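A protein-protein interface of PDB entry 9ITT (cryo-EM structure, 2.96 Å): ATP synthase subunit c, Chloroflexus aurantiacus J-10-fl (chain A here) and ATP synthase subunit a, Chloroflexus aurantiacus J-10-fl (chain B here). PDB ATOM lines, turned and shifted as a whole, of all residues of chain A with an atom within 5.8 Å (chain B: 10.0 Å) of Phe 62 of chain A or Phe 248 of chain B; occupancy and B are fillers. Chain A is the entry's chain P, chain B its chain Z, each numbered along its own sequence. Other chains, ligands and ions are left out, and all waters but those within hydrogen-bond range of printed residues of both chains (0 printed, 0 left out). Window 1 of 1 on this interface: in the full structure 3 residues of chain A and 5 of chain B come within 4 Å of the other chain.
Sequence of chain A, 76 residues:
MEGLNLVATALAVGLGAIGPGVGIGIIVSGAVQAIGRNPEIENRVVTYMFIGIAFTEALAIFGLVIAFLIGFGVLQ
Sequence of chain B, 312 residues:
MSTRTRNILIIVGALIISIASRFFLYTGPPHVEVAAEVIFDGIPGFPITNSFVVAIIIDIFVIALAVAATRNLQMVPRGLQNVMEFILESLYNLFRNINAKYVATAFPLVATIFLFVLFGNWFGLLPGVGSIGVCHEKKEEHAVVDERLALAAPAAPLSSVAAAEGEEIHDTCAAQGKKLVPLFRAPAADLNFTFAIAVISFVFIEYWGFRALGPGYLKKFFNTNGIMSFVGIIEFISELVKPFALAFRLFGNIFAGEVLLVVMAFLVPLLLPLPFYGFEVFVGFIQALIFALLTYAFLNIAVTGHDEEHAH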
ATOM      1  N   GLU A  57      -0.863  -9.280  14.788  1.00  0.00           N
ATOM      2  CA  GLU A  57       0.146 -10.225  14.334  1.00  0.00           C
ATOM      3  C   GLU A  57      -0.115 -10.678  12.904  1.00  0.00           C
ATOM      4  O   GLU A  57       0.824 -11.030  12.192  1.00  0.00           O
ATOM      5  CB  GLU A  57       0.202 -11.431  15.272  1.00  0.00           C
ATOM      6  CG  GLU A  57       1.162 -11.253  16.436  1.00  0.00           C
ATOM      7  CD  GLU A  57       1.404 -12.540  17.194  1.00  0.00           C
ATOM      8  OE1 GLU A  57       0.542 -13.440  17.130  1.00  0.00           O
ATOM      9  OE2 GLU A  57       2.460 -12.652  17.851  1.00  0.00           O
ATOM     10  N   ALA A  58      -1.372 -10.660  12.461  1.00  0.00           N
ATOM     11  CA  ALA A  58      -1.682 -11.005  11.080  1.00  0.00           C
ATOM     12  C   ALA A  58      -1.168  -9.942  10.124  1.00  0.00           C
ATOM     13  O   ALA A  58      -0.629 -10.264   9.059  1.00  0.00           O
ATOM     14  CB  ALA A  58      -3.188 -11.184  10.914  1.00  0.00           C
ATOM     15  N   LEU A  59      -1.342  -8.669  10.476  1.00  0.00           N
ATOM     16  CA  LEU A  59      -0.752  -7.612   9.655  1.00  0.00           C
ATOM     17  C   LEU A  59       0.770  -7.735   9.625  1.00  0.00           C
ATOM     18  O   LEU A  59       1.400  -7.631   8.556  1.00  0.00           O
ATOM     19  CB  LEU A  59      -1.174  -6.239  10.179  1.00  0.00           C
ATOM     20  CG  LEU A  59      -2.683  -6.004  10.303  1.00  0.00           C
ATOM     21  CD1 LEU A  59      -2.955  -4.627  10.879  1.00  0.00           C
ATOM     22  CD2 LEU A  59      -3.379  -6.171   8.959  1.00  0.00           C
ATOM     23  N   ALA A  60       1.374  -7.990  10.789  1.00  0.00           N
ATOM     24  CA  ALA A  60       2.817  -8.203  10.838  1.00  0.00           C
ATOM     25  C   ALA A  60       3.227  -9.379   9.961  1.00  0.00           C
ATOM     26  O   ALA A  60       4.253  -9.327   9.278  1.00  0.00           O
ATOM     27  CB  ALA A  60       3.267  -8.437  12.280  1.00  0.00           C
ATOM     28  N   ILE A  61       2.432 -10.447   9.968  1.00  0.00           N
ATOM     29  CA  ILE A  61       2.759 -11.644   9.205  1.00  0.00           C
ATOM     30  C   ILE A  61       2.619 -11.384   7.712  1.00  0.00           C
ATOM     31  O   ILE A  61       3.368 -11.941   6.905  1.00  0.00           O
ATOM     32  CB  ILE A  61       1.876 -12.815   9.676  1.00  0.00           C
ATOM     33  CG1 ILE A  61       2.399 -13.394  10.999  1.00  0.00           C
ATOM     34  CG2 ILE A  61       1.810 -13.912   8.631  1.00  0.00           C
ATOM     35  CD1 ILE A  61       3.685 -14.208  10.887  1.00  0.00           C
ATOM     36  N   PHE A  62       1.638 -10.571   7.315  1.00  0.00           N
ATOM     37  CA  PHE A  62       1.557 -10.159   5.917  1.00  0.00           C
ATOM     38  C   PHE A  62       2.838  -9.452   5.501  1.00  0.00           C
ATOM     39  O   PHE A  62       3.425  -9.763   4.452  1.00  0.00           O
ATOM     40  CB  PHE A  62       0.355  -9.236   5.695  1.00  0.00           C
ATOM     41  CG  PHE A  62      -0.975  -9.844   6.056  1.00  0.00           C
ATOM     42  CD1 PHE A  62      -1.197 -11.208   5.956  1.00  0.00           C
ATOM     43  CD2 PHE A  62      -2.014  -9.036   6.489  1.00  0.00           C
ATOM     44  CE1 PHE A  62      -2.423 -11.747   6.287  1.00  0.00           C
ATOM     45  CE2 PHE A  62      -3.241  -9.573   6.823  1.00  0.00           C
ATOM     46  CZ  PHE A  62      -3.446 -10.931   6.721  1.00  0.00           C
ATOM     47  N   GLY A  63       3.298  -8.511   6.328  1.00  0.00           N
ATOM     48  CA  GLY A  63       4.573  -7.867   6.047  1.00  0.00           C
ATOM     49  C   GLY A  63       5.716  -8.862   5.950  1.00  0.00           C
ATOM     50  O   GLY A  63       6.539  -8.794   5.033  1.00  0.00           O
ATOM     51  N   LEU A  64       5.764  -9.813   6.884  1.00  0.00           N
ATOM     52  CA  LEU A  64       6.846 -10.794   6.919  1.00  0.00           C
ATOM     53  C   LEU A  64       6.859 -11.662   5.667  1.00  0.00           C
ATOM     54  O   LEU A  64       7.916 -11.890   5.069  1.00  0.00           O
ATOM     55  CB  LEU A  64       6.708 -11.666   8.168  1.00  0.00           C
ATOM     56  CG  LEU A  64       6.969 -11.014   9.529  1.00  0.00           C
ATOM     57  CD1 LEU A  64       6.549 -11.935  10.643  1.00  0.00           C
ATOM     58  CD2 LEU A  64       8.441 -10.697   9.701  1.00  0.00           C
ATOM     59  N   VAL A  65       5.696 -12.175   5.266  1.00  0.00           N
ATOM     60  CA  VAL A  65       5.655 -13.076   4.119  1.00  0.00           C
ATOM     61  C   VAL A  65       5.971 -12.318   2.842  1.00  0.00           C
ATOM     62  O   VAL A  65       6.617 -12.855   1.936  1.00  0.00           O
ATOM     63  CB  VAL A  65       4.300 -13.803   4.024  1.00  0.00           C
ATOM     64  CG1 VAL A  65       4.071 -14.660   5.254  1.00  0.00           C
ATOM     65  CG2 VAL A  65       3.145 -12.829   3.803  1.00  0.00           C
ATOM     66  N   ILE A  66       5.521 -11.065   2.735  1.00  0.00           N
ATOM     67  CA  ILE A  66       5.869 -10.285   1.553  1.00  0.00           C
ATOM     68  C   ILE A  66       7.372 -10.028   1.514  1.00  0.00           C
ATOM     69  O   ILE A  66       8.001 -10.091   0.450  1.00  0.00           O
ATOM     70  CB  ILE A  66       5.056  -8.980   1.517  1.00  0.00           C
ATOM     71  CG1 ILE A  66       3.562  -9.291   1.323  1.00  0.00           C
ATOM     72  CG2 ILE A  66       5.586  -8.056   0.423  1.00  0.00           C
ATOM     73  CD1 ILE A  66       3.173  -9.788  -0.068  1.00  0.00           C
ATOM     74  N   ALA A  67       7.975  -9.752   2.674  1.00  0.00           N
ATOM     75  CA  ALA A  67       9.423  -9.584   2.728  1.00  0.00           C
ATOM     76  C   ALA A  67      10.140 -10.860   2.303  1.00  0.00           C
ATOM     77  O   ALA A  67      11.123 -10.810   1.555  1.00  0.00           O
ATOM     78  CB  ALA A  67       9.852  -9.177   4.137  1.00  0.00           C
ATOM     79  N   ALA B 188      -1.454 -25.800   5.996  1.00  0.00           N
ATOM     80  CA  ALA B 188      -1.644 -24.355   5.973  1.00  0.00           C
ATOM     81  C   ALA B 188      -0.578 -23.649   5.149  1.00  0.00           C
ATOM     82  O   ALA B 188      -0.828 -22.550   4.646  1.00  0.00           O
ATOM     83  CB  ALA B 188      -1.650 -23.806   7.398  1.00  0.00           C
ATOM     84  N   ALA B 189       0.600 -24.257   4.989  1.00  0.00           N
ATOM     85  CA  ALA B 189       1.640 -23.672   4.153  1.00  0.00           C
ATOM     86  C   ALA B 189       1.250 -23.621   2.682  1.00  0.00           C
ATOM     87  O   ALA B 189       1.903 -22.907   1.914  1.00  0.00           O
ATOM     88  CB  ALA B 189       2.943 -24.456   4.313  1.00  0.00           C
ATOM     89  N   ASP B 190       0.214 -24.350   2.276  1.00  0.00           N
ATOM     90  CA  ASP B 190      -0.277 -24.335   0.906  1.00  0.00           C
ATOM     91  C   ASP B 190      -1.438 -23.356   0.800  1.00  0.00           C
ATOM     92  O   ASP B 190      -2.402 -23.442   1.568  1.00  0.00           O
ATOM     93  CB  ASP B 190      -0.723 -25.733   0.476  1.00  0.00           C
ATOM     94  N   LEU B 191      -1.340 -22.426  -0.153  1.00  0.00           N
ATOM     95  CA  LEU B 191      -2.437 -21.494  -0.389  1.00  0.00           C
ATOM     96  C   LEU B 191      -3.692 -22.225  -0.847  1.00  0.00           C
ATOM     97  O   LEU B 191      -4.813 -21.785  -0.569  1.00  0.00           O
ATOM     98  CB  LEU B 191      -2.023 -20.449  -1.425  1.00  0.00           C
ATOM     99  N   ASN B 192      -3.521 -23.347  -1.553  1.00  0.00           N
ATOM    100  CA  ASN B 192      -4.662 -24.090  -2.075  1.00  0.00           C
ATOM    101  C   ASN B 192      -5.598 -24.563  -0.969  1.00  0.00           C
ATOM    102  O   ASN B 192      -6.802 -24.706  -1.210  1.00  0.00           O
ATOM    103  CB  ASN B 192      -4.169 -25.290  -2.887  1.00  0.00           C
ATOM    104  N   PHE B 193      -5.074 -24.809   0.232  1.00  0.00           N
ATOM    105  CA  PHE B 193      -5.885 -25.244   1.363  1.00  0.00           C
ATOM    106  C   PHE B 193      -6.502 -24.068   2.113  1.00  0.00           C
ATOM    107  O   PHE B 193      -7.691 -24.097   2.451  1.00  0.00           O
ATOM    108  CB  PHE B 193      -5.033 -26.083   2.321  1.00  0.00           C
ATOM    109  N   THR B 194      -5.703 -23.040   2.404  1.00  0.00           N
ATOM    110  CA  THR B 194      -6.223 -21.891   3.137  1.00  0.00           C
ATOM    111  C   THR B 194      -7.315 -21.186   2.344  1.00  0.00           C
ATOM    112  O   THR B 194      -8.351 -20.805   2.903  1.00  0.00           O
ATOM    113  CB  THR B 194      -5.091 -20.920   3.471  1.00  0.00           C
ATOM    114  N   PHE B 195      -7.108 -21.012   1.036  1.00  0.00           N
ATOM    115  CA  PHE B 195      -8.149 -20.419   0.205  1.00  0.00           C
ATOM    116  C   PHE B 195      -9.381 -21.313   0.155  1.00  0.00           C
ATOM    117  O   PHE B 195     -10.508 -20.816   0.076  1.00  0.00           O
ATOM    118  CB  PHE B 195      -7.620 -20.159  -1.204  1.00  0.00           C
ATOM    119  N   ALA B 196      -9.186 -22.632   0.199  1.00  0.00           N
ATOM    120  CA  ALA B 196     -10.327 -23.542   0.211  1.00  0.00           C
ATOM    121  C   ALA B 196     -11.168 -23.346   1.466  1.00  0.00           C
ATOM    122  O   ALA B 196     -12.399 -23.244   1.393  1.00  0.00           O
ATOM    123  CB  ALA B 196      -9.845 -24.988   0.107  1.00  0.00           C
ATOM    124  N   ILE B 197     -10.517 -23.279   2.628  1.00  0.00           N
ATOM    125  CA  ILE B 197     -11.260 -23.053   3.866  1.00  0.00           C
ATOM    126  C   ILE B 197     -11.929 -21.685   3.834  1.00  0.00           C
ATOM    127  O   ILE B 197     -13.076 -21.529   4.269  1.00  0.00           O
ATOM    128  CB  ILE B 197     -10.344 -23.203   5.097  1.00  0.00           C
ATOM    129  N   ALA B 198     -11.223 -20.672   3.325  1.00  0.00           N
ATOM    130  CA  ALA B 198     -11.786 -19.326   3.291  1.00  0.00           C
ATOM    131  C   ALA B 198     -13.023 -19.262   2.405  1.00  0.00           C
ATOM    132  O   ALA B 198     -14.035 -18.667   2.789  1.00  0.00           O
ATOM    133  CB  ALA B 198     -10.733 -18.329   2.811  1.00  0.00           C
ATOM    134  N   VAL B 199     -12.968 -19.871   1.218  1.00  0.00           N
ATOM    135  CA  VAL B 199     -14.123 -19.831   0.327  1.00  0.00           C
ATOM    136  C   VAL B 199     -15.259 -20.682   0.879  1.00  0.00           C
ATOM    137  O   VAL B 199     -16.434 -20.339   0.707  1.00  0.00           O
ATOM    138  CB  VAL B 199     -13.727 -20.245  -1.105  1.00  0.00           C
ATOM    139  N   VAL B 241     -13.366  -8.728   1.192  1.00  0.00           N
ATOM    140  CA  VAL B 241     -11.982  -8.827   1.651  1.00  0.00           C
ATOM    141  C   VAL B 241     -11.824  -9.956   2.665  1.00  0.00           C
ATOM    142  O   VAL B 241     -10.776 -10.612   2.716  1.00  0.00           O
ATOM    143  CB  VAL B 241     -11.527  -7.473   2.228  1.00  0.00           C
ATOM    144  N   LYS B 242     -12.847 -10.184   3.494  1.00  0.00           N
ATOM    145  CA  LYS B 242     -12.726 -11.091   4.638  1.00  0.00           C
ATOM    146  C   LYS B 242     -12.156 -12.467   4.307  1.00  0.00           C
ATOM    147  O   LYS B 242     -11.210 -12.894   4.991  1.00  0.00           O
ATOM    148  CB  LYS B 242     -14.101 -11.254   5.302  1.00  0.00           C
ATOM    149  N   PRO B 243     -12.661 -13.211   3.313  1.00  0.00           N
ATOM    150  CA  PRO B 243     -12.084 -14.545   3.059  1.00  0.00           C
ATOM    151  C   PRO B 243     -10.626 -14.505   2.639  1.00  0.00           C
ATOM    152  O   PRO B 243      -9.825 -15.325   3.112  1.00  0.00           O
ATOM    153  CB  PRO B 243     -12.986 -15.109   1.950  1.00  0.00           C
ATOM    154  N   PHE B 244     -10.255 -13.572   1.757  1.00  0.00           N
ATOM    155  CA  PHE B 244      -8.855 -13.446   1.365  1.00  0.00           C
ATOM    156  C   PHE B 244      -7.991 -13.096   2.567  1.00  0.00           C
ATOM    157  O   PHE B 244      -6.881 -13.624   2.720  1.00  0.00           O
ATOM    158  CB  PHE B 244      -8.701 -12.376   0.281  1.00  0.00           C
ATOM    159  N   ALA B 245      -8.482 -12.202   3.427  1.00  0.00           N
ATOM    160  CA  ALA B 245      -7.731 -11.823   4.616  1.00  0.00           C
ATOM    161  C   ALA B 245      -7.495 -13.029   5.516  1.00  0.00           C
ATOM    162  O   ALA B 245      -6.376 -13.254   5.985  1.00  0.00           O
ATOM    163  CB  ALA B 245      -8.472 -10.721   5.372  1.00  0.00           C
ATOM    164  N   LEU B 246      -8.540 -13.825   5.757  1.00  0.00           N
ATOM    165  CA  LEU B 246      -8.393 -15.000   6.615  1.00  0.00           C
ATOM    166  C   LEU B 246      -7.419 -16.005   6.008  1.00  0.00           C
ATOM    167  O   LEU B 246      -6.561 -16.567   6.708  1.00  0.00           O
ATOM    168  CB  LEU B 246      -9.759 -15.649   6.843  1.00  0.00           C
ATOM    169  N   ALA B 247      -7.545 -16.250   4.701  1.00  0.00           N
ATOM    170  CA  ALA B 247      -6.674 -17.215   4.038  1.00  0.00           C
ATOM    171  C   ALA B 247      -5.217 -16.783   4.129  1.00  0.00           C
ATOM    172  O   ALA B 247      -4.345 -17.574   4.512  1.00  0.00           O
ATOM    173  CB  ALA B 247      -7.091 -17.381   2.577  1.00  0.00           C
ATOM    174  N   PHE B 248      -4.934 -15.526   3.775  1.00  0.00           N
ATOM    175  CA  PHE B 248      -3.565 -15.035   3.850  1.00  0.00           C
ATOM    176  C   PHE B 248      -3.059 -15.056   5.283  1.00  0.00           C
ATOM    177  O   PHE B 248      -1.901 -15.403   5.530  1.00  0.00           O
ATOM    178  CB  PHE B 248      -3.478 -13.618   3.271  1.00  0.00           C
ATOM    179  N   ARG B 249      -3.918 -14.700   6.244  1.00  0.00           N
ATOM    180  CA  ARG B 249      -3.532 -14.733   7.650  1.00  0.00           C
ATOM    181  C   ARG B 249      -3.026 -16.114   8.038  1.00  0.00           C
ATOM    182  O   ARG B 249      -1.888 -16.261   8.497  1.00  0.00           O
ATOM    183  CB  ARG B 249      -4.729 -14.320   8.514  1.00  0.00           C
ATOM    184  N   LEU B 250      -3.860 -17.139   7.859  1.00  0.00           N
ATOM    185  CA  LEU B 250      -3.468 -18.477   8.293  1.00  0.00           C
ATOM    186  C   LEU B 250      -2.254 -18.975   7.514  1.00  0.00           C
ATOM    187  O   LEU B 250      -1.281 -19.477   8.106  1.00  0.00           O
ATOM    188  CB  LEU B 250      -4.648 -19.441   8.140  1.00  0.00           C
ATOM    189  N   PHE B 251      -2.287 -18.829   6.184  1.00  0.00           N
ATOM    190  CA  PHE B 251      -1.192 -19.320   5.355  1.00  0.00           C
ATOM    191  C   PHE B 251       0.128 -18.694   5.767  1.00  0.00           C
ATOM    192  O   PHE B 251       1.127 -19.396   5.960  1.00  0.00           O
ATOM    193  CB  PHE B 251      -1.476 -19.028   3.881  1.00  0.00           C
ATOM    194  N   GLY B 252       0.154 -17.370   5.905  1.00  0.00           N
ATOM    195  CA  GLY B 252       1.382 -16.709   6.290  1.00  0.00           C
ATOM    196  C   GLY B 252       1.820 -17.079   7.691  1.00  0.00           C
ATOM    197  O   GLY B 252       2.998 -17.327   7.937  1.00  0.00           O
ATOM    198  N   ASN B 253       0.874 -17.135   8.628  1.00  0.00           N
ATOM    199  CA  ASN B 253       1.259 -17.360  10.012  1.00  0.00           C
ATOM    200  C   ASN B 253       1.788 -18.767  10.239  1.00  0.00           C
ATOM    201  O   ASN B 253       2.467 -18.997  11.246  1.00  0.00           O
ATOM    202  CB  ASN B 253       0.082 -17.076  10.941  1.00  0.00           C
ATOM    203  N   ILE B 254       1.501 -19.705   9.340  1.00  0.00           N
ATOM    204  CA  ILE B 254       2.130 -21.026   9.423  1.00  0.00           C
ATOM    205  C   ILE B 254       3.403 -21.098   8.578  1.00  0.00           C
ATOM    206  O   ILE B 254       4.422 -21.649   9.012  1.00  0.00           O
ATOM    207  CB  ILE B 254       1.117 -22.122   9.027  1.00  0.00           C
ATOM    208  N   PHE B 255       3.381 -20.542   7.362  1.00  0.00           N
ATOM    209  CA  PHE B 255       4.546 -20.644   6.487  1.00  0.00           C
ATOM    210  C   PHE B 255       5.730 -19.854   7.034  1.00  0.00           C
ATOM    211  O   PHE B 255       6.874 -20.318   6.970  1.00  0.00           O
ATOM    212  CB  PHE B 255       4.185 -20.163   5.082  1.00  0.00           C
ATOM    213  N   ALA B 256       5.481 -18.653   7.561  1.00  0.00           N
ATOM    214  CA  ALA B 256       6.556 -17.865   8.149  1.00  0.00           C
ATOM    215  C   ALA B 256       7.128 -18.555   9.378  1.00  0.00           C
ATOM    216  O   ALA B 256       8.333 -18.487   9.629  1.00  0.00           O
ATOM    217  CB  ALA B 256       6.048 -16.469   8.507  1.00  0.00           C
ATOM    218  N   GLN B 287      -3.857 -19.329  16.105  1.00  0.00           N
ATOM    219  CA  GLN B 287      -4.393 -19.198  14.753  1.00  0.00           C
ATOM    220  C   GLN B 287      -5.574 -20.132  14.536  1.00  0.00           C
ATOM    221  O   GLN B 287      -6.602 -19.731  13.972  1.00  0.00           O
ATOM    222  CB  GLN B 287      -3.298 -19.479  13.726  1.00  0.00           C
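Of the printed residues of chain B, Phe 62 of chain A touches Ala 245, Phe 248 and Arg 249. Of chain B, only Gly 252 (3.3 Å) and Asn 253 (3.4 Å) come within 4 Å of Ile 61 of chain A. No residue of chain B comes within 4 Å of Gly 63 of chain A. Of the printed residues of chain B, Val 65 of chain A touches Gly 252 (3.5 Å). Printed residues of chain A within 4 Å of Gly 252 of chain B: Ile 61 (3.3 Å) and Val 65 (3.5 Å). Printed residues of chain A within 4 Å of Arg 249 of chain B: Phe 62 (3.3 Å). The nearest residue of chain A that does not touch Phe 248 of chain B is Ile 61 of chain A (5.1 Å).
Ile 61 of chain A touches Gly 252 of chain B (CG2 to C, 3.3 Å). Ile 61 of chain A touches Asn 253 of chain B. Phe 62 of chain A touches Ala 245 of chain B (CZ to O, 3.8 Å). C of Phe 248 of chain B touches CE1 of Phe 62 of chain A, 3.5 Å away. CE1 of Phe 62 of chain A touches N of Arg 249 of chain B, 3.3 Å away. CA of Gly 252 of chain B touches CG1 of Val 65 of chain A, at 3.5 Å.
Hydrophobic or aromatic side chains of chain A within 4 Å of the printed part of chain B: Ile 61, Phe 62 and Val 65. Hydrophobic or aromatic side chains of chain B that line the printed part of chain A: Phe 248. Among the printed residues, 6 pairs touch across the chains. Among the printed residues, no Asp or Glu carboxylate lies within 4 Å of a Lys or Arg side-chain nitrogen of the other chain.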
